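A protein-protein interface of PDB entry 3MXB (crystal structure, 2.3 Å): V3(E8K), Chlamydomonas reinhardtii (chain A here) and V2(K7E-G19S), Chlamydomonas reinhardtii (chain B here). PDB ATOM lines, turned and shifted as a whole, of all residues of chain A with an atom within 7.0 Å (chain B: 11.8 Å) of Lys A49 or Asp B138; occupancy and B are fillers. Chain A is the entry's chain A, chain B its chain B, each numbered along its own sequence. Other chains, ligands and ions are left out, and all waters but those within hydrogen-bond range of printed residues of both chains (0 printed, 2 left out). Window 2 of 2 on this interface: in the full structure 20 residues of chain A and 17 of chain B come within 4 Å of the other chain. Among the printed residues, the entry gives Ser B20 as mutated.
NZ of Lys A49 lies within salt-bridge range of OD1 of Asp B138, 3.3 Å away.
The guanidinium group (NH2) of Arg A52 is in salt-bridge range of the side-chain carboxylate (OD2) of Asp B138 (3.0 Å).
Of the 26 printed residues of chain B, 2 touch a printed residue of chain A.
Hydrophobic or aromatic side chains of chain B that line the printed part of chain A: Leu B98.
Along chain A the printed residues that touch a printed residue of chain B span positions 48 to 54.
Among the printed residues, 6 pairs touch across the chains.
Among the printed residues, Asp or Glu carboxylates within 4 Å of a Lys or Arg side-chain nitrogen of the other chain: Lys A49 with Asp B138 and Arg A52 with Asp B138.
NE of Arg A52 is in hydrogen-bond range of OE1 of Gln A48 (2.8 Å).
The backbone NH of Ser A75 sits at hydrogen-bond distance from the backbone carbonyl oxygen of Gln A48 (2.8 Å).
NZ of Lys A49 is in hydrogen-bond range of OE1 of Gln A51 (3.1 Å).
The side-chain carboxylate (OD2) of Asp B19 is in hydrogen-bond range of the backbone NH (N) of Leu B98 (3.0 Å).
The backbone carbonyl oxygen (O) of Asp B138 is in hydrogen-bond range of the side-chain amino group (NZ) of Lys B140, 2.7 Å away.
Among the printed residues, merely in contact across the chains: Gln A48 with Leu B98 (3.5 Å), Gln A51 with Asp B138 (3.8 Å), Arg A52 with Leu B98 (3.9 Å) and Trp A54 with Leu B98 (3.9 Å).
Of chain B, only Leu B98 comes within 4 Å of Gln A48.
Lys A49 touches just one residue of chain B: Asp B138.
No residue of chain B comes within 4 Å of Thr A50.
Printed residues of chain B within 4 Å of Gln A51: Asp B138 (3.8 Å).
Of the printed residues of chain B, Arg A52 touches Leu B98 (3.9 Å) and Asp B138 (3.0 Å).
Of the printed residues of chain B, Trp A54 touches Leu B98.
No residue of chain B comes within 4 Å of Ser A73.
No residue of chain B comes within 4 Å of Val A74.
No residue of chain B comes within 4 Å of Ser A75.
Printed residues of chain A within 4 Å of Leu B98: Gln A48 (3.5 Å), Arg A52 (3.9 Å) and Trp A54 (3.9 Å).
Asp B138 touches three residues of chain A.
The nearest residue of chain B that does not touch Lys A49 is Asn B137 (6.3 Å).
The nearest residue of chain A that does not touch Asp B138 is Gln A48 (6.2 Å).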
ATOM      1  N   THR A  47      20.039   8.601  12.340  1.00  0.00           N
ATOM      2  CA  THR A  47      21.136   9.535  12.104  1.00  0.00           C
ATOM      3  C   THR A  47      20.732  10.703  11.205  1.00  0.00           C
ATOM      4  O   THR A  47      20.056  10.516  10.202  1.00  0.00           O
ATOM      5  CB  THR A  47      22.347   8.824  11.449  1.00  0.00           C
ATOM      6  OG1 THR A  47      22.727   7.695  12.234  1.00  0.00           O
ATOM      7  CG2 THR A  47      23.531   9.772  11.357  1.00  0.00           C
ATOM      8  N   GLN A  48      21.167  11.906  11.562  1.00  0.00           N
ATOM      9  CA  GLN A  48      20.915  13.083  10.745  1.00  0.00           C
ATOM     10  C   GLN A  48      21.929  14.173  11.065  1.00  0.00           C
ATOM     11  O   GLN A  48      22.312  14.353  12.210  1.00  0.00           O
ATOM     12  CB  GLN A  48      19.489  13.616  10.958  1.00  0.00           C
ATOM     13  CG  GLN A  48      18.938  14.471   9.818  1.00  0.00           C
ATOM     14  CD  GLN A  48      18.614  13.680   8.556  1.00  0.00           C
ATOM     15  OE1 GLN A  48      18.294  14.263   7.521  1.00  0.00           O
ATOM     16  NE2 GLN A  48      18.714  12.355   8.628  1.00  0.00           N
ATOM     17  N   LYS A  49      22.366  14.876  10.027  1.00  0.00           N
ATOM     18  CA  LYS A  49      23.200  16.066  10.151  1.00  0.00           C
ATOM     19  C   LYS A  49      22.696  16.994  11.267  1.00  0.00           C
ATOM     20  O   LYS A  49      21.490  17.246  11.383  1.00  0.00           O
ATOM     21  CB  LYS A  49      23.193  16.791   8.809  1.00  0.00           C
ATOM     22  CG  LYS A  49      24.198  17.896   8.640  1.00  0.00           C
ATOM     23  CD  LYS A  49      23.916  18.631   7.337  1.00  0.00           C
ATOM     24  CE  LYS A  49      24.989  19.669   7.018  1.00  0.00           C
ATOM     25  NZ  LYS A  49      24.660  20.367   5.765  1.00  0.00           N
ATOM     26  N   THR A  50      23.625  17.511  12.068  1.00  0.00           N
ATOM     27  CA  THR A  50      23.286  18.297  13.260  1.00  0.00           C
ATOM     28  C   THR A  50      22.466  19.548  12.937  1.00  0.00           C
ATOM     29  O   THR A  50      21.692  20.034  13.770  1.00  0.00           O
ATOM     30  CB  THR A  50      24.549  18.654  14.095  1.00  0.00           C
ATOM     31  OG1 THR A  50      25.220  17.446  14.470  1.00  0.00           O
ATOM     32  CG2 THR A  50      24.175  19.434  15.374  1.00  0.00           C
ATOM     33  N   GLN A  51      22.622  20.057  11.722  1.00  0.00           N
ATOM     34  CA  GLN A  51      21.786  21.160  11.249  1.00  0.00           C
ATOM     35  C   GLN A  51      20.306  20.779  11.361  1.00  0.00           C
ATOM     36  O   GLN A  51      19.430  21.628  11.508  1.00  0.00           O
ATOM     37  CB  GLN A  51      22.137  21.481   9.799  1.00  0.00           C
ATOM     38  CG  GLN A  51      21.172  22.419   9.089  1.00  0.00           C
ATOM     39  CD  GLN A  51      21.317  22.356   7.572  1.00  0.00           C
ATOM     40  OE1 GLN A  51      22.222  21.696   7.047  1.00  0.00           O
ATOM     41  NE2 GLN A  51      20.424  23.039   6.860  1.00  0.00           N
ATOM     42  N   ARG A  52      20.025  19.488  11.278  1.00  0.00           N
ATOM     43  CA  ARG A  52      18.648  19.030  11.381  1.00  0.00           C
ATOM     44  C   ARG A  52      18.388  18.319  12.709  1.00  0.00           C
ATOM     45  O   ARG A  52      17.574  17.422  12.776  1.00  0.00           O
ATOM     46  CB  ARG A  52      18.297  18.129  10.193  1.00  0.00           C
ATOM     47  CG  ARG A  52      18.120  18.881   8.870  1.00  0.00           C
ATOM     48  CD  ARG A  52      17.680  17.973   7.699  1.00  0.00           C
ATOM     49  NE  ARG A  52      18.716  17.029   7.267  1.00  0.00           N
ATOM     50  CZ  ARG A  52      19.752  17.342   6.487  1.00  0.00           C
ATOM     51  NH1 ARG A  52      19.912  18.595   6.071  1.00  0.00           N
ATOM     52  NH2 ARG A  52      20.643  16.408   6.137  1.00  0.00           N
ATOM     53  N   ARG A  53      19.087  18.723  13.762  1.00  0.00           N
ATOM     54  CA  ARG A  53      18.919  18.086  15.071  1.00  0.00           C
ATOM     55  C   ARG A  53      17.477  18.177  15.564  1.00  0.00           C
ATOM     56  O   ARG A  53      16.968  17.237  16.185  1.00  0.00           O
ATOM     57  CB  ARG A  53      19.851  18.721  16.101  1.00  0.00           C
ATOM     58  CG  ARG A  53      20.168  17.830  17.284  1.00  0.00           C
ATOM     59  CD  ARG A  53      20.755  18.656  18.429  1.00  0.00           C
ATOM     60  NE  ARG A  53      20.113  18.319  19.697  1.00  0.00           N
ATOM     61  CZ  ARG A  53      20.672  17.575  20.649  1.00  0.00           C
ATOM     62  NH1 ARG A  53      21.901  17.103  20.484  1.00  0.00           N
ATOM     63  NH2 ARG A  53      20.008  17.307  21.768  1.00  0.00           N
ATOM     64  N   TRP A  54      16.831  19.316  15.295  1.00  0.00           N
ATOM     65  CA  TRP A  54      15.431  19.536  15.670  1.00  0.00           C
ATOM     66  C   TRP A  54      14.562  18.359  15.230  1.00  0.00           C
ATOM     67  O   TRP A  54      13.644  17.955  15.931  1.00  0.00           O
ATOM     68  CB  TRP A  54      14.899  20.856  15.081  1.00  0.00           C
ATOM     69  CG  TRP A  54      14.916  20.908  13.582  1.00  0.00           C
ATOM     70  CD1 TRP A  54      15.922  21.388  12.780  1.00  0.00           C
ATOM     71  CD2 TRP A  54      13.890  20.436  12.696  1.00  0.00           C
ATOM     72  NE1 TRP A  54      15.581  21.239  11.453  1.00  0.00           N
ATOM     73  CE2 TRP A  54      14.340  20.661  11.375  1.00  0.00           C
ATOM     74  CE3 TRP A  54      12.640  19.842  12.890  1.00  0.00           C
ATOM     75  CZ2 TRP A  54      13.577  20.321  10.265  1.00  0.00           C
ATOM     76  CZ3 TRP A  54      11.887  19.500  11.788  1.00  0.00           C
ATOM     77  CH2 TRP A  54      12.356  19.742  10.488  1.00  0.00           C
ATOM     78  N   LEU A  56      15.469  15.173  14.955  1.00  0.00           N
ATOM     79  CA  LEU A  56      15.677  14.123  15.958  1.00  0.00           C
ATOM     80  C   LEU A  56      15.014  14.470  17.306  1.00  0.00           C
ATOM     81  O   LEU A  56      14.416  13.609  17.942  1.00  0.00           O
ATOM     82  CB  LEU A  56      17.178  13.859  16.151  1.00  0.00           C
ATOM     83  CG  LEU A  56      17.947  13.594  14.854  1.00  0.00           C
ATOM     84  CD1 LEU A  56      19.391  13.296  15.152  1.00  0.00           C
ATOM     85  CD2 LEU A  56      17.313  12.446  14.061  1.00  0.00           C
ATOM     86  N   SER A  73      29.730  16.549  13.204  1.00  0.00           N
ATOM     87  CA  SER A  73      28.763  17.366  12.469  1.00  0.00           C
ATOM     88  C   SER A  73      27.439  16.617  12.320  1.00  0.00           C
ATOM     89  O   SER A  73      26.555  17.019  11.566  1.00  0.00           O
ATOM     90  CB  SER A  73      29.311  17.714  11.079  1.00  0.00           C
ATOM     91  OG  SER A  73      29.555  16.542  10.311  1.00  0.00           O
ATOM     92  N   VAL A  74      27.311  15.524  13.051  1.00  0.00           N
ATOM     93  CA  VAL A  74      26.190  14.626  12.861  1.00  0.00           C
ATOM     94  C   VAL A  74      25.581  14.294  14.215  1.00  0.00           C
ATOM     95  O   VAL A  74      26.289  14.186  15.218  1.00  0.00           O
ATOM     96  CB  VAL A  74      26.655  13.357  12.092  1.00  0.00           C
ATOM     97  CG1 VAL A  74      25.685  12.237  12.230  1.00  0.00           C
ATOM     98  CG2 VAL A  74      26.891  13.681  10.610  1.00  0.00           C
ATOM     99  N   SER A  75      24.261  14.165  14.250  1.00  0.00           N
ATOM    100  CA  SER A  75      23.571  13.829  15.489  1.00  0.00           C
ATOM    101  C   SER A  75      22.819  12.512  15.297  1.00  0.00           C
ATOM    102  O   SER A  75      22.631  12.077  14.166  1.00  0.00           O
ATOM    103  CB  SER A  75      22.610  14.954  15.886  1.00  0.00           C
ATOM    104  OG  SER A  75      23.322  16.116  16.284  1.00  0.00           O
ATOM    105  N   VAL B  18      11.863   9.108   1.083  1.00  0.00           N
ATOM    106  CA  VAL B  18      12.356  10.203   0.255  1.00  0.00           C
ATOM    107  C   VAL B  18      13.095  11.266   1.082  1.00  0.00           C
ATOM    108  O   VAL B  18      14.220  11.688   0.734  1.00  0.00           O
ATOM    109  CB  VAL B  18      11.224  10.847  -0.565  1.00  0.00           C
ATOM    110  CG1 VAL B  18      11.633  12.253  -1.094  1.00  0.00           C
ATOM    111  CG2 VAL B  18      10.812   9.924  -1.695  1.00  0.00           C
ATOM    112  N   ASP B  19      12.461  11.684   2.173  1.00  0.00           N
ATOM    113  CA  ASP B  19      13.083  12.571   3.155  1.00  0.00           C
ATOM    114  C   ASP B  19      14.431  12.029   3.683  1.00  0.00           C
ATOM    115  O   ASP B  19      15.290  12.810   4.086  1.00  0.00           O
ATOM    116  CB  ASP B  19      12.125  12.802   4.351  1.00  0.00           C
ATOM    117  CG  ASP B  19      11.126  13.934   4.105  1.00  0.00           C
ATOM    118  OD1 ASP B  19      11.284  14.680   3.116  1.00  0.00           O
ATOM    119  OD2 ASP B  19      10.186  14.081   4.915  1.00  0.00           O
ATOM    120  N   SER B  20      14.596  10.702   3.717  1.00  0.00           N
ATOM    121  CA  SER B  20      15.846  10.097   4.189  1.00  0.00           C
ATOM    122  C   SER B  20      16.851   9.862   3.053  1.00  0.00           C
ATOM    123  O   SER B  20      17.928  10.430   3.055  1.00  0.00           O
ATOM    124  CB  SER B  20      15.610   8.802   4.992  1.00  0.00           C
ATOM    125  OG  SER B  20      14.889   7.811   4.266  1.00  0.00           O
ATOM    126  N   ASP B  21      16.489   9.062   2.056  1.00  0.00           N
ATOM    127  CA  ASP B  21      17.461   8.647   1.041  1.00  0.00           C
ATOM    128  C   ASP B  21      17.220   9.244  -0.315  1.00  0.00           C
ATOM    129  O   ASP B  21      17.874   8.853  -1.273  1.00  0.00           O
ATOM    130  CB  ASP B  21      17.431   7.130   0.885  1.00  0.00           C
ATOM    131  CG  ASP B  21      18.377   6.434   1.820  1.00  0.00           C
ATOM    132  OD1 ASP B  21      19.239   7.116   2.411  1.00  0.00           O
ATOM    133  OD2 ASP B  21      18.265   5.204   1.952  1.00  0.00           O
ATOM    134  N   GLY B  22      16.264  10.163  -0.414  1.00  0.00           N
ATOM    135  CA  GLY B  22      15.868  10.684  -1.703  1.00  0.00           C
ATOM    136  C   GLY B  22      16.381  12.087  -1.920  1.00  0.00           C
ATOM    137  O   GLY B  22      17.139  12.609  -1.105  1.00  0.00           O
ATOM    138  N   SER B  23      15.969  12.699  -3.023  1.00  0.00           N
ATOM    139  CA  SER B  23      16.513  13.991  -3.418  1.00  0.00           C
ATOM    140  C   SER B  23      15.640  14.693  -4.443  1.00  0.00           C
ATOM    141  O   SER B  23      15.234  14.101  -5.445  1.00  0.00           O
ATOM    142  CB  SER B  23      17.939  13.849  -3.989  1.00  0.00           C
ATOM    143  OG  SER B  23      18.479  15.144  -4.228  1.00  0.00           O
ATOM    144  N   ILE B  24      15.373  15.966  -4.185  1.00  0.00           N
ATOM    145  CA  ILE B  24      14.599  16.772  -5.095  1.00  0.00           C
ATOM    146  C   ILE B  24      15.513  17.837  -5.644  1.00  0.00           C
ATOM    147  O   ILE B  24      16.011  18.682  -4.907  1.00  0.00           O
ATOM    148  CB  ILE B  24      13.345  17.380  -4.422  1.00  0.00           C
ATOM    149  CG1 ILE B  24      12.477  16.259  -3.842  1.00  0.00           C
ATOM    150  CG2 ILE B  24      12.560  18.215  -5.434  1.00  0.00           C
ATOM    151  CD1 ILE B  24      11.143  16.733  -3.226  1.00  0.00           C
ATOM    152  N   ILE B  25      15.734  17.764  -6.949  1.00  0.00           N
ATOM    153  CA  ILE B  25      16.815  18.472  -7.604  1.00  0.00           C
ATOM    154  C   ILE B  25      16.282  19.403  -8.700  1.00  0.00           C
ATOM    155  O   ILE B  25      15.475  18.998  -9.529  1.00  0.00           O
ATOM    156  CB  ILE B  25      17.795  17.457  -8.245  1.00  0.00           C
ATOM    157  CG1 ILE B  25      18.151  16.350  -7.245  1.00  0.00           C
ATOM    158  CG2 ILE B  25      19.053  18.139  -8.746  1.00  0.00           C
ATOM    159  CD1 ILE B  25      18.980  15.214  -7.848  1.00  0.00           C
ATOM    160  N   ALA B  26      16.730  20.651  -8.679  1.00  0.00           N
ATOM    161  CA  ALA B  26      16.480  21.592  -9.763  1.00  0.00           C
ATOM    162  C   ALA B  26      17.825  22.115 -10.279  1.00  0.00           C
ATOM    163  O   ALA B  26      18.709  22.480  -9.486  1.00  0.00           O
ATOM    164  CB  ALA B  26      15.605  22.747  -9.286  1.00  0.00           C
ATOM    165  N   LEU B  98      11.071  16.880   5.530  1.00  0.00           N
ATOM    166  CA  LEU B  98      12.334  17.575   5.292  1.00  0.00           C
ATOM    167  C   LEU B  98      12.401  18.238   3.908  1.00  0.00           C
ATOM    168  O   LEU B  98      13.119  19.217   3.720  1.00  0.00           O
ATOM    169  CB  LEU B  98      13.545  16.641   5.515  1.00  0.00           C
ATOM    170  CG  LEU B  98      13.750  16.056   6.919  1.00  0.00           C
ATOM    171  CD1 LEU B  98      14.969  15.121   6.967  1.00  0.00           C
ATOM    172  CD2 LEU B  98      13.881  17.148   7.967  1.00  0.00           C
ATOM    173  N   LYS B  99      11.667  17.706   2.937  1.00  0.00           N
ATOM    174  CA  LYS B  99      11.758  18.210   1.573  1.00  0.00           C
ATOM    175  C   LYS B  99      10.448  18.813   1.064  1.00  0.00           C
ATOM    176  O   LYS B  99      10.250  18.948  -0.141  1.00  0.00           O
ATOM    177  CB  LYS B  99      12.225  17.086   0.631  1.00  0.00           C
ATOM    178  CG  LYS B  99      13.609  16.521   0.976  1.00  0.00           C
ATOM    179  CD  LYS B  99      13.982  15.338   0.084  1.00  0.00           C
ATOM    180  CE  LYS B  99      15.312  14.706   0.515  1.00  0.00           C
ATOM    181  NZ  LYS B  99      16.439  15.662   0.355  1.00  0.00           N
ATOM    182  N   GLN B 102      11.005  22.068  -1.092  1.00  0.00           N
ATOM    183  CA  GLN B 102      11.639  21.778  -2.371  1.00  0.00           C
ATOM    184  C   GLN B 102      10.562  21.300  -3.342  1.00  0.00           C
ATOM    185  O   GLN B 102      10.502  21.733  -4.494  1.00  0.00           O
ATOM    186  CB  GLN B 102      12.729  20.694  -2.218  1.00  0.00           C
ATOM    187  CG  GLN B 102      14.029  21.130  -1.499  1.00  0.00           C
ATOM    188  CD  GLN B 102      14.021  20.810  -0.005  1.00  0.00           C
ATOM    189  OE1 GLN B 102      13.046  21.092   0.681  1.00  0.00           O
ATOM    190  NE2 GLN B 102      15.118  20.224   0.502  1.00  0.00           N
ATOM    191  N   VAL B 130      14.957  28.070  -8.354  1.00  0.00           N
ATOM    192  CA  VAL B 130      15.907  26.966  -8.420  1.00  0.00           C
ATOM    193  C   VAL B 130      16.998  27.163  -7.371  1.00  0.00           C
ATOM    194  O   VAL B 130      17.388  26.211  -6.697  1.00  0.00           O
ATOM    195  CB  VAL B 130      16.535  26.836  -9.825  1.00  0.00           C
ATOM    196  CG1 VAL B 130      17.689  25.829  -9.822  1.00  0.00           C
ATOM    197  CG2 VAL B 130      15.477  26.439 -10.841  1.00  0.00           C
ATOM    198  N   ASP B 131      17.478  28.402  -7.232  1.00  0.00           N
ATOM    199  CA  ASP B 131      18.471  28.738  -6.211  1.00  0.00           C
ATOM    200  C   ASP B 131      17.975  28.328  -4.828  1.00  0.00           C
ATOM    201  O   ASP B 131      18.735  27.828  -3.996  1.00  0.00           O
ATOM    202  CB  ASP B 131      18.762  30.245  -6.193  1.00  0.00           C
ATOM    203  CG  ASP B 131      19.564  30.715  -7.396  1.00  0.00           C
ATOM    204  OD1 ASP B 131      19.947  29.886  -8.243  1.00  0.00           O
ATOM    205  OD2 ASP B 131      19.814  31.938  -7.495  1.00  0.00           O
ATOM    206  N   GLN B 132      16.692  28.560  -4.586  1.00  0.00           N
ATOM    207  CA  GLN B 132      16.099  28.283  -3.290  1.00  0.00           C
ATOM    208  C   GLN B 132      16.042  26.791  -3.005  1.00  0.00           C
ATOM    209  O   GLN B 132      16.215  26.367  -1.860  1.00  0.00           O
ATOM    210  CB  GLN B 132      14.694  28.879  -3.206  1.00  0.00           C
ATOM    211  CG  GLN B 132      14.677  30.383  -3.052  1.00  0.00           C
ATOM    212  CD  GLN B 132      13.294  30.976  -3.278  1.00  0.00           C
ATOM    213  OE1 GLN B 132      13.140  31.938  -4.027  1.00  0.00           O
ATOM    214  NE2 GLN B 132      12.281  30.396  -2.636  1.00  0.00           N
ATOM    215  N   ILE B 133      15.786  25.997  -4.039  1.00  0.00           N
ATOM    216  CA  ILE B 133      15.746  24.551  -3.850  1.00  0.00           C
ATOM    217  C   ILE B 133      17.131  24.090  -3.421  1.00  0.00           C
ATOM    218  O   ILE B 133      17.272  23.353  -2.443  1.00  0.00           O
ATOM    219  CB  ILE B 133      15.287  23.798  -5.114  1.00  0.00           C
ATOM    220  CG1 ILE B 133      13.799  24.039  -5.348  1.00  0.00           C
ATOM    221  CG2 ILE B 133      15.555  22.311  -4.970  1.00  0.00           C
ATOM    222  CD1 ILE B 133      13.367  23.973  -6.790  1.00  0.00           C
ATOM    223  N   ALA B 134      18.147  24.570  -4.132  1.00  0.00           N
ATOM    224  CA  ALA B 134      19.527  24.182  -3.860  1.00  0.00           C
ATOM    225  C   ALA B 134      19.939  24.641  -2.468  1.00  0.00           C
ATOM    226  O   ALA B 134      20.704  23.947  -1.788  1.00  0.00           O
ATOM    227  CB  ALA B 134      20.482  24.757  -4.923  1.00  0.00           C
ATOM    228  N   ALA B 135      19.431  25.802  -2.043  1.00  0.00           N
ATOM    229  CA  ALA B 135      19.718  26.305  -0.693  1.00  0.00           C
ATOM    230  C   ALA B 135      19.136  25.396   0.400  1.00  0.00           C
ATOM    231  O   ALA B 135      19.724  25.231   1.463  1.00  0.00           O
ATOM    232  CB  ALA B 135      19.232  27.764  -0.518  1.00  0.00           C
ATOM    233  N   LEU B 136      17.995  24.787   0.121  1.00  0.00           N
ATOM    234  CA  LEU B 136      17.367  23.900   1.089  1.00  0.00           C
ATOM    235  C   LEU B 136      18.065  22.547   1.097  1.00  0.00           C
ATOM    236  O   LEU B 136      18.123  21.873   2.123  1.00  0.00           O
ATOM    237  CB  LEU B 136      15.874  23.728   0.765  1.00  0.00           C
ATOM    238  CG  LEU B 136      15.057  25.017   0.868  1.00  0.00           C
ATOM    239  CD1 LEU B 136      13.776  24.949   0.073  1.00  0.00           C
ATOM    240  CD2 LEU B 136      14.761  25.321   2.339  1.00  0.00           C
ATOM    241  N   ASN B 137      18.573  22.138  -0.056  1.00  0.00           N
ATOM    242  CA  ASN B 137      19.321  20.887  -0.155  1.00  0.00           C
ATOM    243  C   ASN B 137      20.705  20.995   0.517  1.00  0.00           C
ATOM    244  O   ASN B 137      21.150  22.090   0.842  1.00  0.00           O
ATOM    245  CB  ASN B 137      19.508  20.512  -1.627  1.00  0.00           C
ATOM    246  CG  ASN B 137      18.245  19.989  -2.274  1.00  0.00           C
ATOM    247  OD1 ASN B 137      17.253  19.684  -1.603  1.00  0.00           O
ATOM    248  ND2 ASN B 137      18.289  19.848  -3.593  1.00  0.00           N
ATOM    249  N   ASP B 138      21.378  19.864   0.728  1.00  0.00           N
ATOM    250  CA  ASP B 138      22.769  19.898   1.189  1.00  0.00           C
ATOM    251  C   ASP B 138      23.709  20.124  -0.020  1.00  0.00           C
ATOM    252  O   ASP B 138      24.572  19.301  -0.313  1.00  0.00           O
ATOM    253  CB  ASP B 138      23.123  18.589   1.920  1.00  0.00           C
ATOM    254  CG  ASP B 138      22.416  18.448   3.303  1.00  0.00           C
ATOM    255  OD1 ASP B 138      22.101  19.481   3.927  1.00  0.00           O
ATOM    256  OD2 ASP B 138      22.192  17.299   3.780  1.00  0.00           O
ATOM    257  N   SER B 139      23.512  21.227  -0.737  1.00  0.00           N
ATOM    258  CA  SER B 139      24.298  21.529  -1.945  1.00  0.00           C
ATOM    259  C   SER B 139      25.823  21.648  -1.727  1.00  0.00           C
ATOM    260  O   SER B 139      26.256  22.331  -0.813  1.00  0.00           O
ATOM    261  CB  SER B 139      23.794  22.831  -2.560  1.00  0.00           C
ATOM    262  OG  SER B 139      24.380  23.011  -3.824  1.00  0.00           O
ATOM    263  N   LYS B 140      26.624  21.012  -2.585  1.00  0.00           N
ATOM    264  CA  LYS B 140      28.091  20.967  -2.407  1.00  0.00           C
ATOM    265  C   LYS B 140      28.933  21.191  -3.675  1.00  0.00           C
ATOM    266  O   LYS B 140      30.103  21.551  -3.581  1.00  0.00           O
ATOM    267  CB  LYS B 140      28.515  19.634  -1.780  1.00  0.00           C
ATOM    268  CG  LYS B 140      28.415  19.605  -0.278  1.00  0.00           C
ATOM    269  CD  LYS B 140      28.789  18.233   0.268  1.00  0.00           C
ATOM    270  CE  LYS B 140      27.894  17.150  -0.314  1.00  0.00           C
ATOM    271  NZ  LYS B 140      26.459  17.400   0.041  1.00  0.00           N
ATOM    272  N   THR B 141      28.357  20.960  -4.853  1.00  0.00           N
ATOM    273  CA  THR B 141      29.116  21.109  -6.094  1.00  0.00           C
ATOM    274  C   THR B 141      28.353  21.923  -7.137  1.00  0.00           C
ATOM    275  O   THR B 141      28.572  21.775  -8.339  1.00  0.00           O
ATOM    276  CB  THR B 141      29.461  19.744  -6.710  1.00  0.00           C
ATOM    277  OG1 THR B 141      28.245  19.044  -7.001  1.00  0.00           O
ATOM    278  CG2 THR B 141      30.364  18.900  -5.763  1.00  0.00           C
ATOM    279  N   ARG B 142      27.447  22.774  -6.679  1.00  0.00           N
ATOM    280  CA  ARG B 142      26.644  23.562  -7.591  1.00  0.00           C
ATOM    281  C   ARG B 142      27.492  24.607  -8.346  1.00  0.00           C
ATOM    282  O   ARG B 142      28.382  25.219  -7.775  1.00  0.00           O
ATOM    283  CB  ARG B 142      25.503  24.229  -6.834  1.00  0.00           C
ATOM    284  CG  ARG B 142      24.444  24.825  -7.742  1.00  0.00           C
ATOM    285  CD  ARG B 142      23.251  25.291  -6.925  1.00  0.00           C
ATOM    286  NE  ARG B 142      22.247  25.830  -7.817  1.00  0.00           N
ATOM    287  CZ  ARG B 142      21.809  27.080  -7.785  1.00  0.00           C
ATOM    288  NH1 ARG B 142      22.274  27.938  -6.871  1.00  0.00           N
ATOM    289  NH2 ARG B 142      20.902  27.461  -8.672  1.00  0.00           N
ATOM    290  N   LYS B 143      27.206  24.800  -9.630  1.00  0.00           N
ATOM    291  CA  LYS B 143      27.987  25.722 -10.457  1.00  0.00           C
ATOM    292  C   LYS B 143      27.134  26.808 -11.101  1.00  0.00           C
ATOM    293  O   LYS B 143      27.390  27.990 -10.925  1.00  0.00           O
ATOM    294  CB  LYS B 143      28.720  24.963 -11.559  1.00  0.00           C
ATOM    295  CG  LYS B 143      30.041  24.362 -11.135  1.00  0.00           C
ATOM    296  CD  LYS B 143      30.804  23.878 -12.352  1.00  0.00           C
ATOM    297  CE  LYS B 143      30.789  24.928 -13.454  1.00  0.00           C
ATOM    298  NZ  LYS B 143      31.407  24.418 -14.707  1.00  0.00           N
